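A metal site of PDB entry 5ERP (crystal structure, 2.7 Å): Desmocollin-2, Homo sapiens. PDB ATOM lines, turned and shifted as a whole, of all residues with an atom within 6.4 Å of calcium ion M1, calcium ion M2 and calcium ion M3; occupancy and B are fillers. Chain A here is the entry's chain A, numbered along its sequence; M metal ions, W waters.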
ATOM      1  N   GLU A  19     -10.027  29.163  -2.265  1.00  0.00           N
ATOM      2  CA  GLU A  19     -10.326  30.417  -1.586  1.00  0.00           C
ATOM      3  C   GLU A  19     -10.146  30.249  -0.077  1.00  0.00           C
ATOM      4  O   GLU A  19     -10.170  29.123   0.436  1.00  0.00           O
ATOM      5  CB  GLU A  19     -11.748  30.879  -1.910  1.00  0.00           C
ATOM      6  CG  GLU A  19     -12.822  29.899  -1.463  1.00  0.00           C
ATOM      7  CD  GLU A  19     -14.222  30.409  -1.747  1.00  0.00           C
ATOM      8  OE1 GLU A  19     -14.455  31.636  -1.652  1.00  0.00           O
ATOM      9  OE2 GLU A  19     -15.090  29.579  -2.066  1.00  0.00           O
ATOM     10  N   ASN A  20      -9.985  31.368   0.615  1.00  0.00           N
ATOM     11  CA  ASN A  20      -9.817  31.377   2.063  1.00  0.00           C
ATOM     12  C   ASN A  20      -8.564  30.635   2.532  1.00  0.00           C
ATOM     13  O   ASN A  20      -8.429  30.328   3.719  1.00  0.00           O
ATOM     14  CB  ASN A  20     -11.047  30.787   2.750  1.00  0.00           C
ATOM     15  CG  ASN A  20     -12.337  31.410   2.275  1.00  0.00           C
ATOM     16  OD1 ASN A  20     -12.340  32.555   1.815  1.00  0.00           O
ATOM     17  ND2 ASN A  20     -13.442  30.678   2.397  1.00  0.00           N
ATOM     18  N   LEU A  76      -8.793  35.876  -0.378  1.00  0.00           N
ATOM     19  CA  LEU A  76      -9.176  35.407  -1.704  1.00  0.00           C
ATOM     20  C   LEU A  76     -10.607  34.875  -1.637  1.00  0.00           C
ATOM     21  O   LEU A  76     -10.900  33.976  -0.853  1.00  0.00           O
ATOM     22  CB  LEU A  76      -8.216  34.321  -2.182  1.00  0.00           C
ATOM     23  CG  LEU A  76      -6.765  34.760  -2.368  1.00  0.00           C
ATOM     24  CD1 LEU A  76      -5.822  33.597  -2.102  1.00  0.00           C
ATOM     25  CD2 LEU A  76      -6.564  35.337  -3.765  1.00  0.00           C
ATOM     26  N   ASP A  77     -11.475  35.433  -2.473  1.00  0.00           N
ATOM     27  CA  ASP A  77     -12.896  35.115  -2.423  1.00  0.00           C
ATOM     28  C   ASP A  77     -13.445  34.841  -3.815  1.00  0.00           C
ATOM     29  O   ASP A  77     -13.524  35.750  -4.650  1.00  0.00           O
ATOM     30  CB  ASP A  77     -13.671  36.250  -1.756  1.00  0.00           C
ATOM     31  CG  ASP A  77     -15.092  35.856  -1.387  1.00  0.00           C
ATOM     32  OD1 ASP A  77     -15.427  34.663  -1.472  1.00  0.00           O
ATOM     33  OD2 ASP A  77     -15.878  36.749  -1.004  1.00  0.00           O
ATOM     34  N   ARG A  78     -13.818  33.595  -4.057  1.00  0.00           N
ATOM     35  CA  ARG A  78     -14.268  33.148  -5.367  1.00  0.00           C
ATOM     36  C   ARG A  78     -15.532  33.885  -5.802  1.00  0.00           C
ATOM     37  O   ARG A  78     -15.733  34.139  -6.990  1.00  0.00           O
ATOM     38  CB  ARG A  78     -14.531  31.631  -5.344  1.00  0.00           C
ATOM     39  CG  ARG A  78     -14.489  30.981  -6.724  1.00  0.00           C
ATOM     40  CD  ARG A  78     -15.480  29.825  -6.883  1.00  0.00           C
ATOM     41  NE  ARG A  78     -16.654  30.221  -7.649  1.00  0.00           N
ATOM     42  CZ  ARG A  78     -17.855  30.497  -7.139  1.00  0.00           C
ATOM     43  NH1 ARG A  78     -18.079  30.397  -5.836  1.00  0.00           N
ATOM     44  NH2 ARG A  78     -18.824  30.859  -7.959  1.00  0.00           N
ATOM     45  N   GLU A  79     -16.378  34.232  -4.835  1.00  0.00           N
ATOM     46  CA  GLU A  79     -17.655  34.887  -5.115  1.00  0.00           C
ATOM     47  C   GLU A  79     -17.495  36.370  -5.451  1.00  0.00           C
ATOM     48  O   GLU A  79     -18.440  37.016  -5.889  1.00  0.00           O
ATOM     49  CB  GLU A  79     -18.605  34.708  -3.925  1.00  0.00           C
ATOM     50  CG  GLU A  79     -19.178  33.293  -3.798  1.00  0.00           C
ATOM     51  CD  GLU A  79     -18.209  32.302  -3.173  1.00  0.00           C
ATOM     52  OE1 GLU A  79     -17.246  32.736  -2.504  1.00  0.00           O
ATOM     53  OE2 GLU A  79     -18.410  31.080  -3.356  1.00  0.00           O
ATOM     54  N   LEU A  80     -16.293  36.907  -5.223  1.00  0.00           N
ATOM     55  CA  LEU A  80     -15.993  38.301  -5.590  1.00  0.00           C
ATOM     56  C   LEU A  80     -15.118  38.334  -6.840  1.00  0.00           C
ATOM     57  O   LEU A  80     -15.433  39.030  -7.803  1.00  0.00           O
ATOM     58  CB  LEU A  80     -15.297  39.027  -4.440  1.00  0.00           C
ATOM     59  CG  LEU A  80     -16.137  39.274  -3.176  1.00  0.00           C
ATOM     60  CD1 LEU A  80     -15.275  39.838  -2.056  1.00  0.00           C
ATOM     61  CD2 LEU A  80     -17.293  40.218  -3.479  1.00  0.00           C
ATOM     62  N   ASP A 111     -10.485  28.090  -6.737  1.00  0.00           N
ATOM     63  CA  ASP A 111     -11.383  26.965  -6.618  1.00  0.00           C
ATOM     64  C   ASP A 111     -12.384  27.242  -5.507  1.00  0.00           C
ATOM     65  O   ASP A 111     -12.140  28.079  -4.634  1.00  0.00           O
ATOM     66  CB  ASP A 111     -10.600  25.685  -6.335  1.00  0.00           C
ATOM     67  CG  ASP A 111     -11.217  24.455  -6.968  1.00  0.00           C
ATOM     68  OD1 ASP A 111     -12.459  24.407  -7.102  1.00  0.00           O
ATOM     69  OD2 ASP A 111     -10.463  23.536  -7.323  1.00  0.00           O
ATOM     70  N   ASP A 112     -13.516  26.540  -5.525  1.00  0.00           N
ATOM     71  CA  ASP A 112     -14.597  26.808  -4.594  1.00  0.00           C
ATOM     72  C   ASP A 112     -14.520  25.924  -3.343  1.00  0.00           C
ATOM     73  O   ASP A 112     -14.122  24.763  -3.415  1.00  0.00           O
ATOM     74  CB  ASP A 112     -15.949  26.604  -5.282  1.00  0.00           C
ATOM     75  CG  ASP A 112     -17.126  27.017  -4.418  1.00  0.00           C
ATOM     76  OD1 ASP A 112     -17.131  28.175  -3.957  1.00  0.00           O
ATOM     77  OD2 ASP A 112     -18.032  26.181  -4.210  1.00  0.00           O
ATOM     78  N   VAL A 113     -14.890  26.508  -2.205  1.00  0.00           N
ATOM     79  CA  VAL A 113     -15.123  25.747  -0.977  1.00  0.00           C
ATOM     80  C   VAL A 113     -16.506  26.115  -0.473  1.00  0.00           C
ATOM     81  O   VAL A 113     -17.033  27.178  -0.816  1.00  0.00           O
ATOM     82  CB  VAL A 113     -14.050  26.016   0.111  1.00  0.00           C
ATOM     83  CG1 VAL A 113     -12.641  25.881  -0.461  1.00  0.00           C
ATOM     84  CG2 VAL A 113     -14.239  27.390   0.734  1.00  0.00           C
ATOM     85  N   ASN A 114     -17.109  25.248   0.336  1.00  0.00           N
ATOM     86  CA  ASN A 114     -18.470  25.450   0.805  1.00  0.00           C
ATOM     87  C   ASN A 114     -18.534  26.427   1.985  1.00  0.00           C
ATOM     88  O   ASN A 114     -18.482  25.999   3.141  1.00  0.00           O
ATOM     89  CB  ASN A 114     -19.090  24.101   1.198  1.00  0.00           C
ATOM     90  CG  ASN A 114     -20.543  24.219   1.639  1.00  0.00           C
ATOM     91  OD1 ASN A 114     -21.289  25.055   1.145  1.00  0.00           O
ATOM     92  ND2 ASN A 114     -20.939  23.360   2.560  1.00  0.00           N
ATOM     93  N   ASP A 115     -18.631  27.714   1.691  1.00  0.00           N
ATOM     94  CA  ASP A 115     -18.659  28.744   2.736  1.00  0.00           C
ATOM     95  C   ASP A 115     -19.924  29.597   2.694  1.00  0.00           C
ATOM     96  O   ASP A 115     -20.012  30.614   3.393  1.00  0.00           O
ATOM     97  CB  ASP A 115     -17.416  29.638   2.638  1.00  0.00           C
ATOM     98  CG  ASP A 115     -17.218  30.233   1.254  1.00  0.00           C
ATOM     99  OD1 ASP A 115     -17.981  29.899   0.334  1.00  0.00           O
ATOM    100  OD2 ASP A 115     -16.280  31.034   1.107  1.00  0.00           O
ATOM    101  N   HIS A 116     -20.892  29.197   1.879  1.00  0.00           N
ATOM    102  CA  HIS A 116     -22.255  29.744   1.957  1.00  0.00           C
ATOM    103  C   HIS A 116     -23.250  28.627   2.219  1.00  0.00           C
ATOM    104  O   HIS A 116     -23.394  27.711   1.414  1.00  0.00           O
ATOM    105  CB  HIS A 116     -22.633  30.481   0.665  1.00  0.00           C
ATOM    106  CG  HIS A 116     -21.843  31.722   0.409  1.00  0.00           C
ATOM    107  ND1 HIS A 116     -20.678  31.730  -0.328  1.00  0.00           N
ATOM    108  CD2 HIS A 116     -22.063  33.007   0.780  1.00  0.00           C
ATOM    109  CE1 HIS A 116     -20.211  32.961  -0.390  1.00  0.00           C
ATOM    110  NE2 HIS A 116     -21.029  33.759   0.279  1.00  0.00           N
ATOM    111  N   LEU A 117     -23.955  28.694   3.348  1.00  0.00           N
ATOM    112  CA  LEU A 117     -24.975  27.703   3.652  1.00  0.00           C
ATOM    113  C   LEU A 117     -26.205  27.973   2.808  1.00  0.00           C
ATOM    114  O   LEU A 117     -26.567  29.141   2.596  1.00  0.00           O
ATOM    115  CB  LEU A 117     -25.342  27.717   5.135  1.00  0.00           C
ATOM    116  CG  LEU A 117     -24.206  27.374   6.095  1.00  0.00           C
ATOM    117  CD1 LEU A 117     -24.541  27.840   7.502  1.00  0.00           C
ATOM    118  CD2 LEU A 117     -23.967  25.863   6.092  1.00  0.00           C
ATOM    119  N   PRO A 118     -26.875  26.919   2.313  1.00  0.00           N
ATOM    120  CA  PRO A 118     -28.066  27.164   1.505  1.00  0.00           C
ATOM    121  C   PRO A 118     -29.237  27.572   2.384  1.00  0.00           C
ATOM    122  O   PRO A 118     -29.395  27.063   3.489  1.00  0.00           O
ATOM    123  CB  PRO A 118     -28.309  25.822   0.826  1.00  0.00           C
ATOM    124  CG  PRO A 118     -27.798  24.822   1.805  1.00  0.00           C
ATOM    125  CD  PRO A 118     -26.650  25.481   2.535  1.00  0.00           C
ATOM    126  N   ASP A 145     -27.930  29.652  -2.816  1.00  0.00           N
ATOM    127  CA  ASP A 145     -26.591  29.211  -2.457  1.00  0.00           C
ATOM    128  C   ASP A 145     -25.594  29.881  -3.390  1.00  0.00           C
ATOM    129  O   ASP A 145     -25.647  29.687  -4.605  1.00  0.00           O
ATOM    130  CB  ASP A 145     -26.466  27.690  -2.533  1.00  0.00           C
ATOM    131  CG  ASP A 145     -25.252  27.162  -1.791  1.00  0.00           C
ATOM    132  OD1 ASP A 145     -24.161  27.739  -1.941  1.00  0.00           O
ATOM    133  OD2 ASP A 145     -25.400  26.166  -1.055  1.00  0.00           O
ATOM    134  N   LYS A 146     -24.685  30.656  -2.811  1.00  0.00           N
ATOM    135  CA  LYS A 146     -23.768  31.467  -3.596  1.00  0.00           C
ATOM    136  C   LYS A 146     -22.519  30.703  -4.023  1.00  0.00           C
ATOM    137  O   LYS A 146     -21.666  31.253  -4.724  1.00  0.00           O
ATOM    138  CB  LYS A 146     -23.379  32.709  -2.801  1.00  0.00           C
ATOM    139  CG  LYS A 146     -24.472  33.756  -2.781  1.00  0.00           C
ATOM    140  CD  LYS A 146     -24.308  34.752  -1.652  1.00  0.00           C
ATOM    141  CE  LYS A 146     -25.454  35.744  -1.606  1.00  0.00           C
ATOM    142  NZ  LYS A 146     -25.600  36.475  -2.901  1.00  0.00           N
ATOM    143  N   ASP A 147     -22.421  29.441  -3.626  1.00  0.00           N
ATOM    144  CA  ASP A 147     -21.255  28.641  -3.999  1.00  0.00           C
ATOM    145  C   ASP A 147     -21.373  28.212  -5.458  1.00  0.00           C
ATOM    146  O   ASP A 147     -22.350  28.532  -6.129  1.00  0.00           O
ATOM    147  CB  ASP A 147     -21.118  27.423  -3.079  1.00  0.00           C
ATOM    148  CG  ASP A 147     -20.736  27.809  -1.665  1.00  0.00           C
ATOM    149  OD1 ASP A 147     -19.970  28.782  -1.495  1.00  0.00           O
ATOM    150  OD2 ASP A 147     -21.192  27.133  -0.717  1.00  0.00           O
ATOM    151  N   LEU A 148     -20.370  27.491  -5.929  1.00  0.00           N
ATOM    152  CA  LEU A 148     -20.243  27.176  -7.345  1.00  0.00           C
ATOM    153  C   LEU A 148     -21.257  26.129  -7.811  1.00  0.00           C
ATOM    154  O   LEU A 148     -21.338  25.041  -7.241  1.00  0.00           O
ATOM    155  CB  LEU A 148     -18.824  26.714  -7.650  1.00  0.00           C
ATOM    156  CG  LEU A 148     -18.527  26.296  -9.092  1.00  0.00           C
ATOM    157  CD1 LEU A 148     -18.784  27.445 -10.044  1.00  0.00           C
ATOM    158  CD2 LEU A 148     -17.095  25.807  -9.205  1.00  0.00           C
ATOM    159  N   ALA A 152     -20.848  19.718  -4.948  1.00  0.00           N
ATOM    160  CA  ALA A 152     -21.316  19.279  -3.639  1.00  0.00           C
ATOM    161  C   ALA A 152     -21.394  20.443  -2.643  1.00  0.00           C
ATOM    162  O   ALA A 152     -21.980  20.302  -1.570  1.00  0.00           O
ATOM    163  CB  ALA A 152     -20.404  18.185  -3.092  1.00  0.00           C
ATOM    164  N   ASN A 153     -20.791  21.568  -2.994  1.00  0.00           N
ATOM    165  CA  ASN A 153     -20.848  22.765  -2.160  1.00  0.00           C
ATOM    166  C   ASN A 153     -22.103  23.571  -2.442  1.00  0.00           C
ATOM    167  O   ASN A 153     -22.395  24.542  -1.741  1.00  0.00           O
ATOM    168  CB  ASN A 153     -19.623  23.639  -2.404  1.00  0.00           C
ATOM    169  CG  ASN A 153     -18.320  22.920  -2.154  1.00  0.00           C
ATOM    170  OD1 ASN A 153     -18.257  21.964  -1.381  1.00  0.00           O
ATOM    171  ND2 ASN A 153     -17.261  23.359  -2.833  1.00  0.00           N
ATOM    172  N   TRP A 154     -22.851  23.165  -3.461  1.00  0.00           N
ATOM    173  CA  TRP A 154     -23.992  23.931  -3.947  1.00  0.00           C
ATOM    174  C   TRP A 154     -25.316  23.185  -3.831  1.00  0.00           C
ATOM    175  O   TRP A 154     -26.281  23.701  -3.254  1.00  0.00           O
ATOM    176  CB  TRP A 154     -23.763  24.315  -5.409  1.00  0.00           C
ATOM    177  CG  TRP A 154     -24.912  25.008  -6.056  1.00  0.00           C
ATOM    178  CD1 TRP A 154     -25.270  26.318  -5.911  1.00  0.00           C
ATOM    179  CD2 TRP A 154     -25.848  24.442  -6.973  1.00  0.00           C
ATOM    180  NE1 TRP A 154     -26.367  26.597  -6.676  1.00  0.00           N
ATOM    181  CE2 TRP A 154     -26.747  25.469  -7.342  1.00  0.00           C
ATOM    182  CE3 TRP A 154     -26.009  23.173  -7.529  1.00  0.00           C
ATOM    183  CZ2 TRP A 154     -27.796  25.255  -8.231  1.00  0.00           C
ATOM    184  CZ3 TRP A 154     -27.048  22.958  -8.414  1.00  0.00           C
ATOM    185  CH2 TRP A 154     -27.924  23.993  -8.757  1.00  0.00           C
ATOM    186  N   ARG A 155     -25.371  21.978  -4.377  1.00  0.00           N
ATOM    187  CA  ARG A 155     -26.631  21.245  -4.495  1.00  0.00           C
ATOM    188  C   ARG A 155     -27.195  20.847  -3.142  1.00  0.00           C
ATOM    189  O   ARG A 155     -26.454  20.489  -2.226  1.00  0.00           O
ATOM    190  CB  ARG A 155     -26.441  20.005  -5.363  1.00  0.00           C
ATOM    191  CG  ARG A 155     -25.511  18.963  -4.792  1.00  0.00           C
ATOM    192  CD  ARG A 155     -25.427  17.753  -5.716  1.00  0.00           C
ATOM    193  NE  ARG A 155     -24.049  17.392  -6.039  1.00  0.00           N
ATOM    194  CZ  ARG A 155     -23.425  17.715  -7.162  1.00  0.00           C
ATOM    195  NH1 ARG A 155     -24.038  18.425  -8.111  1.00  0.00           N
ATOM    196  NH2 ARG A 155     -22.175  17.333  -7.347  1.00  0.00           N
ATOM    197  N   ASN A 204     -26.065  21.176   2.184  1.00  0.00           N
ATOM    198  CA  ASN A 204     -25.370  20.726   0.974  1.00  0.00           C
ATOM    199  C   ASN A 204     -24.923  19.280   1.157  1.00  0.00           C
ATOM    200  O   ASN A 204     -24.957  18.747   2.264  1.00  0.00           O
ATOM    201  CB  ASN A 204     -24.160  21.602   0.677  1.00  0.00           C
ATOM    202  CG  ASN A 204     -24.502  23.080   0.634  1.00  0.00           C
ATOM    203  OD1 ASN A 204     -24.002  23.858   1.447  1.00  0.00           O
ATOM    204  ND2 ASN A 204     -25.334  23.476  -0.316  1.00  0.00           N
ATOM    205  N   PHE A 208     -20.221  22.330   5.693  1.00  0.00           N
ATOM    206  CA  PHE A 208     -19.815  23.739   5.696  1.00  0.00           C
ATOM    207  C   PHE A 208     -18.287  23.797   5.858  1.00  0.00           C
ATOM    208  O   PHE A 208     -17.703  22.835   6.373  1.00  0.00           O
ATOM    209  CB  PHE A 208     -20.513  24.487   6.843  1.00  0.00           C
ATOM    210  CG  PHE A 208     -20.424  25.983   6.770  1.00  0.00           C
ATOM    211  CD1 PHE A 208     -20.613  26.653   5.565  1.00  0.00           C
ATOM    212  CD2 PHE A 208     -20.162  26.735   7.903  1.00  0.00           C
ATOM    213  CE1 PHE A 208     -20.547  28.039   5.510  1.00  0.00           C
ATOM    214  CE2 PHE A 208     -20.084  28.116   7.841  1.00  0.00           C
ATOM    215  CZ  PHE A 208     -20.277  28.768   6.645  1.00  0.00           C
HETATM  216 CA    CA M   1     -16.190  32.829  -0.353  1.00  0.00          CA
HETATM  217 CA    CA M   2     -17.586  29.410  -1.940  1.00  0.00          CA
HETATM  218 CA    CA M   3     -23.147  26.024  -0.099  1.00  0.00          CA
HETATM  219  O   HOH W   1     -14.325  33.409   0.990  1.00  0.00           O
HETATM  220  O   HOH W   2     -17.818  34.264   0.791  1.00  0.00           O
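The side-chain amide nitrogen of Asn 204 lies within hydrogen-bond range of the backbone carbonyl oxygen of Trp 154 (3.1 Å). The side-chain carboxylate (OD2) of Asp 112 lies within hydrogen-bond range of the backbone NH (N) of Leu 148, 3.2 Å away. OD2 of Asp 112 is in hydrogen-bond range of ND2 of Asn 153 (3.2 Å). A ring nitrogen (ND1) of His 116 lies close to the side-chain carboxylate (OD1) of Asp 115, 3.3 Å away. The side-chain carboxylate (OE2) of Glu 79 lies close to the guanidinium group (NH1) of Arg 78 (2.6 Å). OE1 of Glu 19 sits close to N of Arg 78 (3.2 Å). The guanidinium group (NH1) of Arg 78 lies close to the side-chain carboxylate (OD1) of Asp 112. OD2 of Asp 115 lies close to ND2 of Asn 20 (3.1 Å).
Four residues have an atom within 4 Å of calcium ion M1: Glu 19, Asp 77, Glu 79 and Asp 115. The nearest printed residue that does not touch calcium ion M1 is His 116 (4.02 Å).
Six residues have an atom within 4 Å of calcium ion M2: Glu 19, Glu 79, Asp 112, Val 113, Asp 115 and Asp 147. The nearest printed residue that does not touch calcium ion M2 is Arg 78 (4.05 Å).
Calcium ion M1 is bound by OD1 of Asp 77. Calcium ion M1 is bound by OD2 of Asp 115 (2.3 Å). Calcium ion M1 is bound by water W1, at 2.4 Å. OE1 of Glu 79 is bound to calcium ion M1 (2.4 Å). Calcium ion M1 is bound by water W2 (2.5 Å). The side-chain carboxylate (OE1) of Glu 19 is bound to calcium ion M1 (2.5 Å). Calcium ion M1 has six donor atoms within binding distance.
Calcium ion M2 is bound by the side-chain carboxylate (OE2) of Glu 79, at 2.3 Å. The side-chain carboxylate (OD1) of Asp 115 is bound to calcium ion M2 (2.4 Å). OD1 of Asp 112 binds calcium ion M2. Calcium ion M2 is bound by OE2 of Glu 19 (2.5 Å). Calcium ion M2 is bound by OD1 of Asp 147 (2.5 Å). O of Val 113 is bound to calcium ion M2, at 2.6 Å.
Calcium ion M3 is bound by O of His 116, OD2 of Asp 147, O of Asn 153, OD1 of Asn 114, OD2 of Asp 145, OD1 of Asp 145 and OD1 of Asn 204.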
